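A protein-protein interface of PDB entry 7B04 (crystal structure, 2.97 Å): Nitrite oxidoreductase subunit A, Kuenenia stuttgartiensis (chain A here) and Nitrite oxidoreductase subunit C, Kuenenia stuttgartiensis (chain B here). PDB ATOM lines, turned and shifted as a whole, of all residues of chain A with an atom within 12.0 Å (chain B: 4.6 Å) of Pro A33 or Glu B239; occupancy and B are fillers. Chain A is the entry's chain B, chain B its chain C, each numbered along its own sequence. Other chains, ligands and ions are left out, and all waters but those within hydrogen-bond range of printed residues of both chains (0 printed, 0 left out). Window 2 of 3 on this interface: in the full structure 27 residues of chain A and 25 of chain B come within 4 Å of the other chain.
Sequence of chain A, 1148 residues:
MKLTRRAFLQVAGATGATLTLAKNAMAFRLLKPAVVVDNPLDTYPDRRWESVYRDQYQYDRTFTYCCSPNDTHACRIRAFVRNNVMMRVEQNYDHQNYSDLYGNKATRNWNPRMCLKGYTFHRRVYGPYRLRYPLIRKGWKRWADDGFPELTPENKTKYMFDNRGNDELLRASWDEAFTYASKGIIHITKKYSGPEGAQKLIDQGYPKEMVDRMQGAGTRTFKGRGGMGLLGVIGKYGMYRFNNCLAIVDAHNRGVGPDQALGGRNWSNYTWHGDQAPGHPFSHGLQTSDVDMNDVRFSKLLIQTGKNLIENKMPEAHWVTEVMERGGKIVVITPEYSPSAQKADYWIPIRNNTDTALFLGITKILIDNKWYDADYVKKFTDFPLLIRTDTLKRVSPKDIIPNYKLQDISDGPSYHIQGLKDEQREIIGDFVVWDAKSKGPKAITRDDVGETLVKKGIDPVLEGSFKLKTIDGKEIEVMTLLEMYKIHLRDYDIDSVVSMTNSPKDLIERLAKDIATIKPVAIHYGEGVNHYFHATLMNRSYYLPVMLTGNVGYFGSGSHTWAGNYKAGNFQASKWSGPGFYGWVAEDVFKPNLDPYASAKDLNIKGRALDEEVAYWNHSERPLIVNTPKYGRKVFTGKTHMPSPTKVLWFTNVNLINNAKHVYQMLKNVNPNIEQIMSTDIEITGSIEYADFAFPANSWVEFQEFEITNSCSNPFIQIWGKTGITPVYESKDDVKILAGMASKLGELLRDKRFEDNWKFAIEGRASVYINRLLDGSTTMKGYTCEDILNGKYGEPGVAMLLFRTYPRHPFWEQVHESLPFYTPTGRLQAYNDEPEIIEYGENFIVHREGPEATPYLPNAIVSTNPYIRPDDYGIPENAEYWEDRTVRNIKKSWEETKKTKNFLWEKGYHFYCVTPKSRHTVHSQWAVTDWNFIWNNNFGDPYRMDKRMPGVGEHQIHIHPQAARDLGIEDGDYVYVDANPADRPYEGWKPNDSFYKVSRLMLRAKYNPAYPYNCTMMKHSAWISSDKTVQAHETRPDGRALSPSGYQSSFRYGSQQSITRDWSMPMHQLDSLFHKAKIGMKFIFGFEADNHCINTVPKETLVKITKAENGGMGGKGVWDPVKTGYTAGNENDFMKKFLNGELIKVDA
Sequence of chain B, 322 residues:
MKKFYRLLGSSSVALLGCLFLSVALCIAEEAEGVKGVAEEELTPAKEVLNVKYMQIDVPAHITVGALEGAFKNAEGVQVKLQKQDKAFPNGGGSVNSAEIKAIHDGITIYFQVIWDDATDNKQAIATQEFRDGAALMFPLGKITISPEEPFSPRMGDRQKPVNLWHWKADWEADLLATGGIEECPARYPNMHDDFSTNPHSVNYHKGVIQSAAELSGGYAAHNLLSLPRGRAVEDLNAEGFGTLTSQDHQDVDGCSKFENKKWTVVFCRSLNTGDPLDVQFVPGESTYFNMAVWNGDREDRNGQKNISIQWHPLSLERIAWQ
Glu B239 touches just these residues of chain A: Pro A33 (3.5 Å) and Ala A34 (3.7 Å).
No residue of chain A comes within 4 Å of Gly B156.
No residue of chain A comes within 4 Å of Asp B157.
No residue of chain A comes within 4 Å of Arg B158.
Printed residues of chain A within 4 Å of Asn B237: Pro A33.
No residue of chain A comes within 4 Å of Ala B238.
No residue of chain A comes within 4 Å of Gly B240.
Thr B243 touches two residues of chain A.
Of chain A, only Pro A33 (3.9 Å), Ala A34 (3.1 Å) and Val A35 (2.9 Å) come within 4 Å of Thr B245.
Of chain A, only Leu A31 (3.96 Å) and Pro A33 (3.6 Å) come within 4 Å of Leu B277.
Printed residues of chain B within 4 Å of Ala A34: Glu B239, Thr B243 and Thr B245.
Of the printed residues of chain B, Leu A31 touches Leu B277.
Printed residues of chain A within 4 Å of Pro B161: Pro A33.
Printed residues of chain B within 4 Å of Val A35: Thr B243 (3.8 Å) and Thr B245 (2.9 Å).
Lys A32 touches none of the printed residues of chain B.
The nearest residue of chain A that does not touch Glu B239 is Val A36 (4.3 Å).
Hydrophobic or aromatic side chains of chain B that line the printed part of chain A: Pro B161 and Leu B277.
Of the 13 printed residues of chain A, 4 touch a printed residue of chain B.
Among the printed residues, pairs that only touch across the chains: Leu A31 with Leu B277, Pro A33 with Pro B161, Pro A33 with Asn B237, Pro A33 with Glu B239, Pro A33 with Thr B245, Pro A33 with Leu B277, Ala A34 with Glu B239, Ala A34 with Thr B243, Ala A34 with Thr B245 and Val A35 with Thr B243.
The side-chain hydroxyl (OG1) of Thr B245 sits at hydrogen-bond distance from the backbone NH (N) of Val A35, 2.9 Å away.
The side-chain hydroxyl (OG1) of Thr B245 sits at hydrogen-bond distance from the backbone carbonyl oxygen (O) of Thr B243 (2.8 Å).
NH1 of Arg B158 sits at hydrogen-bond distance from O of Glu B239, 2.9 Å away.
The backbone carbonyl oxygen (O) of Asn B237 lies within hydrogen-bond range of the backbone NH (N) of Thr B245, 2.7 Å away.
The backbone carbonyl oxygen (O) of Leu B277 sits close to the side-chain amide oxygen (OD1) of Asn B237 (3.1 Å).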
ATOM      1  N   PHE A  28      -0.681 -14.846  -0.375  1.00  0.00           N
ATOM      2  CA  PHE A  28      -0.430 -15.099  -1.790  1.00  0.00           C
ATOM      3  C   PHE A  28      -1.124 -14.072  -2.675  1.00  0.00           C
ATOM      4  O   PHE A  28      -0.752 -13.885  -3.831  1.00  0.00           O
ATOM      5  CB  PHE A  28      -0.882 -16.494  -2.160  1.00  0.00           C
ATOM      6  N   ARG A  29      -2.147 -13.434  -2.123  1.00  0.00           N
ATOM      7  CA  ARG A  29      -2.858 -12.403  -2.858  1.00  0.00           C
ATOM      8  C   ARG A  29      -1.958 -11.192  -3.027  1.00  0.00           C
ATOM      9  O   ARG A  29      -1.040 -10.967  -2.230  1.00  0.00           O
ATOM     10  CB  ARG A  29      -4.137 -12.014  -2.126  1.00  0.00           C
ATOM     11  N   LEU A  30      -2.210 -10.423  -4.088  1.00  0.00           N
ATOM     12  CA  LEU A  30      -1.331  -9.306  -4.422  1.00  0.00           C
ATOM     13  C   LEU A  30      -1.251  -8.336  -3.254  1.00  0.00           C
ATOM     14  O   LEU A  30      -2.260  -8.003  -2.626  1.00  0.00           O
ATOM     15  CB  LEU A  30      -1.807  -8.567  -5.674  1.00  0.00           C
ATOM     16  CG  LEU A  30      -0.716  -7.636  -6.236  1.00  0.00           C
ATOM     17  CD1 LEU A  30      -0.447  -7.881  -7.706  1.00  0.00           C
ATOM     18  CD2 LEU A  30      -1.033  -6.168  -5.981  1.00  0.00           C
ATOM     19  N   LEU A  31      -0.032  -7.909  -2.954  1.00  0.00           N
ATOM     20  CA  LEU A  31       0.237  -7.058  -1.811  1.00  0.00           C
ATOM     21  C   LEU A  31       0.069  -5.605  -2.210  1.00  0.00           C
ATOM     22  O   LEU A  31       0.453  -5.210  -3.314  1.00  0.00           O
ATOM     23  CB  LEU A  31       1.657  -7.312  -1.316  1.00  0.00           C
ATOM     24  CG  LEU A  31       1.823  -8.295  -0.160  1.00  0.00           C
ATOM     25  CD1 LEU A  31       1.026  -7.839   1.046  1.00  0.00           C
ATOM     26  CD2 LEU A  31       1.400  -9.684  -0.584  1.00  0.00           C
ATOM     27  N   LYS A  32      -0.512  -4.811  -1.308  1.00  0.00           N
ATOM     28  CA  LYS A  32      -0.507  -3.369  -1.481  1.00  0.00           C
ATOM     29  C   LYS A  32       0.807  -2.894  -0.877  1.00  0.00           C
ATOM     30  O   LYS A  32       0.919  -2.827   0.359  1.00  0.00           O
ATOM     31  CB  LYS A  32      -1.709  -2.737  -0.795  1.00  0.00           C
ATOM     32  CG  LYS A  32      -1.695  -1.224  -0.650  1.00  0.00           C
ATOM     33  CD  LYS A  32      -3.030  -0.760  -0.053  1.00  0.00           C
ATOM     34  CE  LYS A  32      -3.021   0.707   0.372  1.00  0.00           C
ATOM     35  NZ  LYS A  32      -3.913   1.584  -0.446  1.00  0.00           N
ATOM     36  N   PRO A  33       1.818  -2.557  -1.690  1.00  0.00           N
ATOM     37  CA  PRO A  33       3.131  -2.225  -1.114  1.00  0.00           C
ATOM     38  C   PRO A  33       3.102  -0.924  -0.347  1.00  0.00           C
ATOM     39  O   PRO A  33       3.846  -0.756   0.630  1.00  0.00           O
ATOM     40  CB  PRO A  33       4.047  -2.138  -2.349  1.00  0.00           C
ATOM     41  CG  PRO A  33       3.245  -2.775  -3.471  1.00  0.00           C
ATOM     42  CD  PRO A  33       1.835  -2.424  -3.157  1.00  0.00           C
ATOM     43  N   ALA A  34       2.274   0.020  -0.786  1.00  0.00           N
ATOM     44  CA  ALA A  34       2.266   1.347  -0.204  1.00  0.00           C
ATOM     45  C   ALA A  34       0.834   1.856  -0.123  1.00  0.00           C
ATOM     46  O   ALA A  34      -0.035   1.446  -0.897  1.00  0.00           O
ATOM     47  CB  ALA A  34       3.149   2.277  -1.025  1.00  0.00           C
ATOM     48  N   VAL A  35       0.590   2.740   0.838  1.00  0.00           N
ATOM     49  CA  VAL A  35      -0.728   3.327   1.054  1.00  0.00           C
ATOM     50  C   VAL A  35      -0.805   4.663   0.330  1.00  0.00           C
ATOM     51  O   VAL A  35       0.041   5.543   0.532  1.00  0.00           O
ATOM     52  CB  VAL A  35      -1.029   3.485   2.550  1.00  0.00           C
ATOM     53  CG1 VAL A  35      -2.366   4.165   2.738  1.00  0.00           C
ATOM     54  CG2 VAL A  35      -1.012   2.125   3.230  1.00  0.00           C
ATOM     55  N   VAL A  36      -1.831   4.817  -0.502  1.00  0.00           N
ATOM     56  CA  VAL A  36      -2.030   6.007  -1.317  1.00  0.00           C
ATOM     57  C   VAL A  36      -3.238   6.768  -0.788  1.00  0.00           C
ATOM     58  O   VAL A  36      -4.291   6.175  -0.519  1.00  0.00           O
ATOM     59  CB  VAL A  36      -2.251   5.633  -2.793  1.00  0.00           C
ATOM     60  CG1 VAL A  36      -2.373   6.876  -3.653  1.00  0.00           C
ATOM     61  CG2 VAL A  36      -1.133   4.701  -3.282  1.00  0.00           C
ATOM     62  N   VAL A  37      -3.079   8.081  -0.619  1.00  0.00           N
ATOM     63  CA  VAL A  37      -4.144   8.970  -0.174  1.00  0.00           C
ATOM     64  C   VAL A  37      -4.372   9.996  -1.279  1.00  0.00           C
ATOM     65  O   VAL A  37      -3.410  10.567  -1.812  1.00  0.00           O
ATOM     66  CB  VAL A  37      -3.791   9.665   1.153  1.00  0.00           C
ATOM     67  CG1 VAL A  37      -4.987  10.437   1.672  1.00  0.00           C
ATOM     68  CG2 VAL A  37      -3.313   8.646   2.181  1.00  0.00           C
ATOM     69  N   ASP A  38      -5.641  10.244  -1.618  1.00  0.00           N
ATOM     70  CA  ASP A  38      -5.955  11.130  -2.751  1.00  0.00           C
ATOM     71  C   ASP A  38      -6.193  12.567  -2.294  1.00  0.00           C
ATOM     72  O   ASP A  38      -5.409  13.467  -2.611  1.00  0.00           O
ATOM     73  CB  ASP A  38      -7.170  10.596  -3.513  1.00  0.00           C
ATOM     74  CG  ASP A  38      -6.880   9.302  -4.240  1.00  0.00           C
ATOM     75  OD1 ASP A  38      -5.713   9.092  -4.629  1.00  0.00           O
ATOM     76  OD2 ASP A  38      -7.820   8.501  -4.432  1.00  0.00           O
ATOM     77  N   PRO A  45      -8.041   6.498   3.102  1.00  0.00           N
ATOM     78  CA  PRO A  45      -8.058   5.073   2.769  1.00  0.00           C
ATOM     79  C   PRO A  45      -8.405   4.200   3.951  1.00  0.00           C
ATOM     80  O   PRO A  45      -9.237   3.297   3.830  1.00  0.00           O
ATOM     81  CB  PRO A  45      -6.623   4.807   2.291  1.00  0.00           C
ATOM     82  CG  PRO A  45      -6.106   6.141   1.899  1.00  0.00           C
ATOM     83  CD  PRO A  45      -6.728   7.104   2.852  1.00  0.00           C
ATOM     84  N   ASP A  46      -7.711   4.394   5.058  1.00  0.00           N
ATOM     85  CA  ASP A  46      -7.923   3.487   6.213  1.00  0.00           C
ATOM     86  C   ASP A  46      -8.071   4.282   7.506  1.00  0.00           C
ATOM     87  O   ASP A  46      -7.187   5.050   7.802  1.00  0.00           O
ATOM     88  CB  ASP A  46      -6.747   2.518   6.251  1.00  0.00           C
ATOM     89  CG  ASP A  46      -6.840   1.436   7.280  1.00  0.00           C
ATOM     90  OD1 ASP A  46      -7.863   1.332   7.860  1.00  0.00           O
ATOM     91  OD2 ASP A  46      -5.876   0.738   7.466  1.00  0.00           O
ATOM     92  N   MET B 155      11.507   8.402  -5.196  1.00  0.00           N
ATOM     93  CA  MET B 155      10.944   7.373  -4.317  1.00  0.00           C
ATOM     94  C   MET B 155       9.983   6.449  -5.063  1.00  0.00           C
ATOM     95  O   MET B 155       8.944   6.047  -4.537  1.00  0.00           O
ATOM     96  CB  MET B 155      10.241   8.001  -3.113  1.00  0.00           C
ATOM     97  CG  MET B 155      11.137   8.794  -2.196  1.00  0.00           C
ATOM     98  SD  MET B 155      10.154   9.649  -0.957  1.00  0.00           S
ATOM     99  CE  MET B 155       9.624   8.282   0.067  1.00  0.00           C
ATOM    100  N   GLY B 156      10.335   6.096  -6.295  1.00  0.00           N
ATOM    101  CA  GLY B 156       9.470   5.246  -7.089  1.00  0.00           C
ATOM    102  C   GLY B 156       8.367   6.019  -7.790  1.00  0.00           C
ATOM    103  O   GLY B 156       8.406   7.248  -7.921  1.00  0.00           O
ATOM    104  N   ASP B 157       7.363   5.273  -8.247  1.00  0.00           N
ATOM    105  CA  ASP B 157       6.177   5.866  -8.853  1.00  0.00           C
ATOM    106  C   ASP B 157       5.037   4.854  -8.798  1.00  0.00           C
ATOM    107  O   ASP B 157       5.214   3.711  -8.367  1.00  0.00           O
ATOM    108  CB  ASP B 157       6.473   6.307 -10.291  1.00  0.00           C
ATOM    109  CG  ASP B 157       5.466   7.311 -10.816  1.00  0.00           C
ATOM    110  OD1 ASP B 157       4.528   7.657 -10.070  1.00  0.00           O
ATOM    111  OD2 ASP B 157       5.618   7.754 -11.975  1.00  0.00           O
ATOM    112  N   ARG B 158       3.853   5.298  -9.223  1.00  0.00           N
ATOM    113  CA  ARG B 158       2.643   4.498  -9.079  1.00  0.00           C
ATOM    114  C   ARG B 158       2.724   3.231  -9.925  1.00  0.00           C
ATOM    115  O   ARG B 158       3.161   3.263 -11.078  1.00  0.00           O
ATOM    116  CB  ARG B 158       1.418   5.314  -9.490  1.00  0.00           C
ATOM    117  CG  ARG B 158       1.301   6.656  -8.796  1.00  0.00           C
ATOM    118  CD  ARG B 158       1.106   6.492  -7.298  1.00  0.00           C
ATOM    119  NE  ARG B 158       0.787   7.761  -6.649  1.00  0.00           N
ATOM    120  CZ  ARG B 158       1.696   8.611  -6.180  1.00  0.00           C
ATOM    121  NH1 ARG B 158       2.989   8.330  -6.284  1.00  0.00           N
ATOM    122  NH2 ARG B 158       1.313   9.743  -5.605  1.00  0.00           N
ATOM    123  N   GLN B 159       2.322   2.105  -9.332  1.00  0.00           N
ATOM    124  CA  GLN B 159       2.422   0.781  -9.950  1.00  0.00           C
ATOM    125  C   GLN B 159       3.867   0.408 -10.256  1.00  0.00           C
ATOM    126  O   GLN B 159       4.127  -0.489 -11.064  1.00  0.00           O
ATOM    127  CB  GLN B 159       1.559   0.670 -11.217  1.00  0.00           C
ATOM    128  CG  GLN B 159       0.064   0.672 -10.943  1.00  0.00           C
ATOM    129  CD  GLN B 159      -0.636   1.882 -11.525  1.00  0.00           C
ATOM    130  OE1 GLN B 159      -0.337   2.310 -12.640  1.00  0.00           O
ATOM    131  NE2 GLN B 159      -1.577   2.441 -10.771  1.00  0.00           N
ATOM    132  N   LYS B 160       4.807   1.097  -9.616  1.00  0.00           N
ATOM    133  CA  LYS B 160       6.238   0.826  -9.754  1.00  0.00           C
ATOM    134  C   LYS B 160       6.854   0.939  -8.367  1.00  0.00           C
ATOM    135  O   LYS B 160       7.522   1.927  -8.039  1.00  0.00           O
ATOM    136  CB  LYS B 160       6.885   1.793 -10.750  1.00  0.00           C
ATOM    137  CG  LYS B 160       6.432   1.590 -12.193  1.00  0.00           C
ATOM    138  CD  LYS B 160       7.130   2.551 -13.143  1.00  0.00           C
ATOM    139  CE  LYS B 160       6.780   2.251 -14.594  1.00  0.00           C
ATOM    140  NZ  LYS B 160       5.348   2.533 -14.900  1.00  0.00           N
ATOM    141  N   PRO B 161       6.636  -0.063  -7.516  1.00  0.00           N
ATOM    142  CA  PRO B 161       7.040   0.043  -6.108  1.00  0.00           C
ATOM    143  C   PRO B 161       8.549  -0.023  -5.928  1.00  0.00           C
ATOM    144  O   PRO B 161       9.302  -0.432  -6.813  1.00  0.00           O
ATOM    145  CB  PRO B 161       6.352  -1.157  -5.454  1.00  0.00           C
ATOM    146  CG  PRO B 161       6.242  -2.154  -6.555  1.00  0.00           C
ATOM    147  CD  PRO B 161       6.022  -1.365  -7.818  1.00  0.00           C
ATOM    148  N   ASN B 237       8.591   0.622   2.253  1.00  0.00           N
ATOM    149  CA  ASN B 237       8.303   0.657   0.825  1.00  0.00           C
ATOM    150  C   ASN B 237       7.663   1.980   0.425  1.00  0.00           C
ATOM    151  O   ASN B 237       7.139   2.719   1.263  1.00  0.00           O
ATOM    152  CB  ASN B 237       7.362  -0.485   0.413  1.00  0.00           C
ATOM    153  CG  ASN B 237       8.082  -1.799   0.226  1.00  0.00           C
ATOM    154  OD1 ASN B 237       7.948  -2.714   1.036  1.00  0.00           O
ATOM    155  ND2 ASN B 237       8.848  -1.903  -0.853  1.00  0.00           N
ATOM    156  N   ALA B 238       7.711   2.269  -0.876  1.00  0.00           N
ATOM    157  CA  ALA B 238       7.063   3.456  -1.421  1.00  0.00           C
ATOM    158  C   ALA B 238       6.751   3.235  -2.897  1.00  0.00           C
ATOM    159  O   ALA B 238       7.489   2.549  -3.610  1.00  0.00           O
ATOM    160  CB  ALA B 238       7.932   4.705  -1.239  1.00  0.00           C
ATOM    161  N   GLU B 239       5.640   3.830  -3.338  1.00  0.00           N
ATOM    162  CA  GLU B 239       5.253   3.878  -4.745  1.00  0.00           C
ATOM    163  C   GLU B 239       5.216   5.329  -5.211  1.00  0.00           C
ATOM    164  O   GLU B 239       4.250   5.760  -5.851  1.00  0.00           O
ATOM    165  CB  GLU B 239       3.891   3.210  -4.969  1.00  0.00           C
ATOM    166  CG  GLU B 239       3.918   1.693  -5.075  1.00  0.00           C
ATOM    167  CD  GLU B 239       2.530   1.106  -5.292  1.00  0.00           C
ATOM    168  OE1 GLU B 239       1.538   1.825  -5.047  1.00  0.00           O
ATOM    169  OE2 GLU B 239       2.426  -0.069  -5.702  1.00  0.00           O
ATOM    170  N   GLY B 240       6.249   6.084  -4.870  1.00  0.00           N
ATOM    171  CA  GLY B 240       6.292   7.512  -5.104  1.00  0.00           C
ATOM    172  C   GLY B 240       6.432   8.273  -3.800  1.00  0.00           C
ATOM    173  O   GLY B 240       6.312   7.725  -2.703  1.00  0.00           O
ATOM    174  N   THR B 243       3.966   8.684  -0.459  1.00  0.00           N
ATOM    175  CA  THR B 243       3.388   7.352  -0.405  1.00  0.00           C
ATOM    176  C   THR B 243       4.217   6.412   0.468  1.00  0.00           C
ATOM    177  O   THR B 243       3.889   5.221   0.592  1.00  0.00           O
ATOM    178  CB  THR B 243       3.254   6.873  -1.865  1.00  0.00           C
ATOM    179  OG1 THR B 243       2.227   7.637  -2.508  1.00  0.00           O
ATOM    180  CG2 THR B 243       2.887   5.435  -2.015  1.00  0.00           C
ATOM    181  N   THR B 245       5.633   4.030   3.080  1.00  0.00           N
ATOM    182  CA  THR B 245       4.880   3.135   3.944  1.00  0.00           C
ATOM    183  C   THR B 245       5.854   2.254   4.698  1.00  0.00           C
ATOM    184  O   THR B 245       6.798   1.725   4.110  1.00  0.00           O
ATOM    185  CB  THR B 245       3.916   2.263   3.125  1.00  0.00           C
ATOM    186  OG1 THR B 245       3.123   3.096   2.266  1.00  0.00           O
ATOM    187  CG2 THR B 245       2.999   1.489   4.031  1.00  0.00           C
ATOM    188  N   LEU B 277       7.818  -8.020  -0.558  1.00  0.00           N
ATOM    189  CA  LEU B 277       7.988  -6.583  -0.750  1.00  0.00           C
ATOM    190  C   LEU B 277       9.419  -6.135  -0.489  1.00  0.00           C
ATOM    191  O   LEU B 277       9.671  -4.930  -0.389  1.00  0.00           O
ATOM    192  CB  LEU B 277       7.030  -5.797   0.153  1.00  0.00           C
ATOM    193  CG  LEU B 277       5.530  -5.952  -0.095  1.00  0.00           C
ATOM    194  CD1 LEU B 277       4.732  -5.185   0.951  1.00  0.00           C
ATOM    195  CD2 LEU B 277       5.166  -5.494  -1.497  1.00  0.00           C
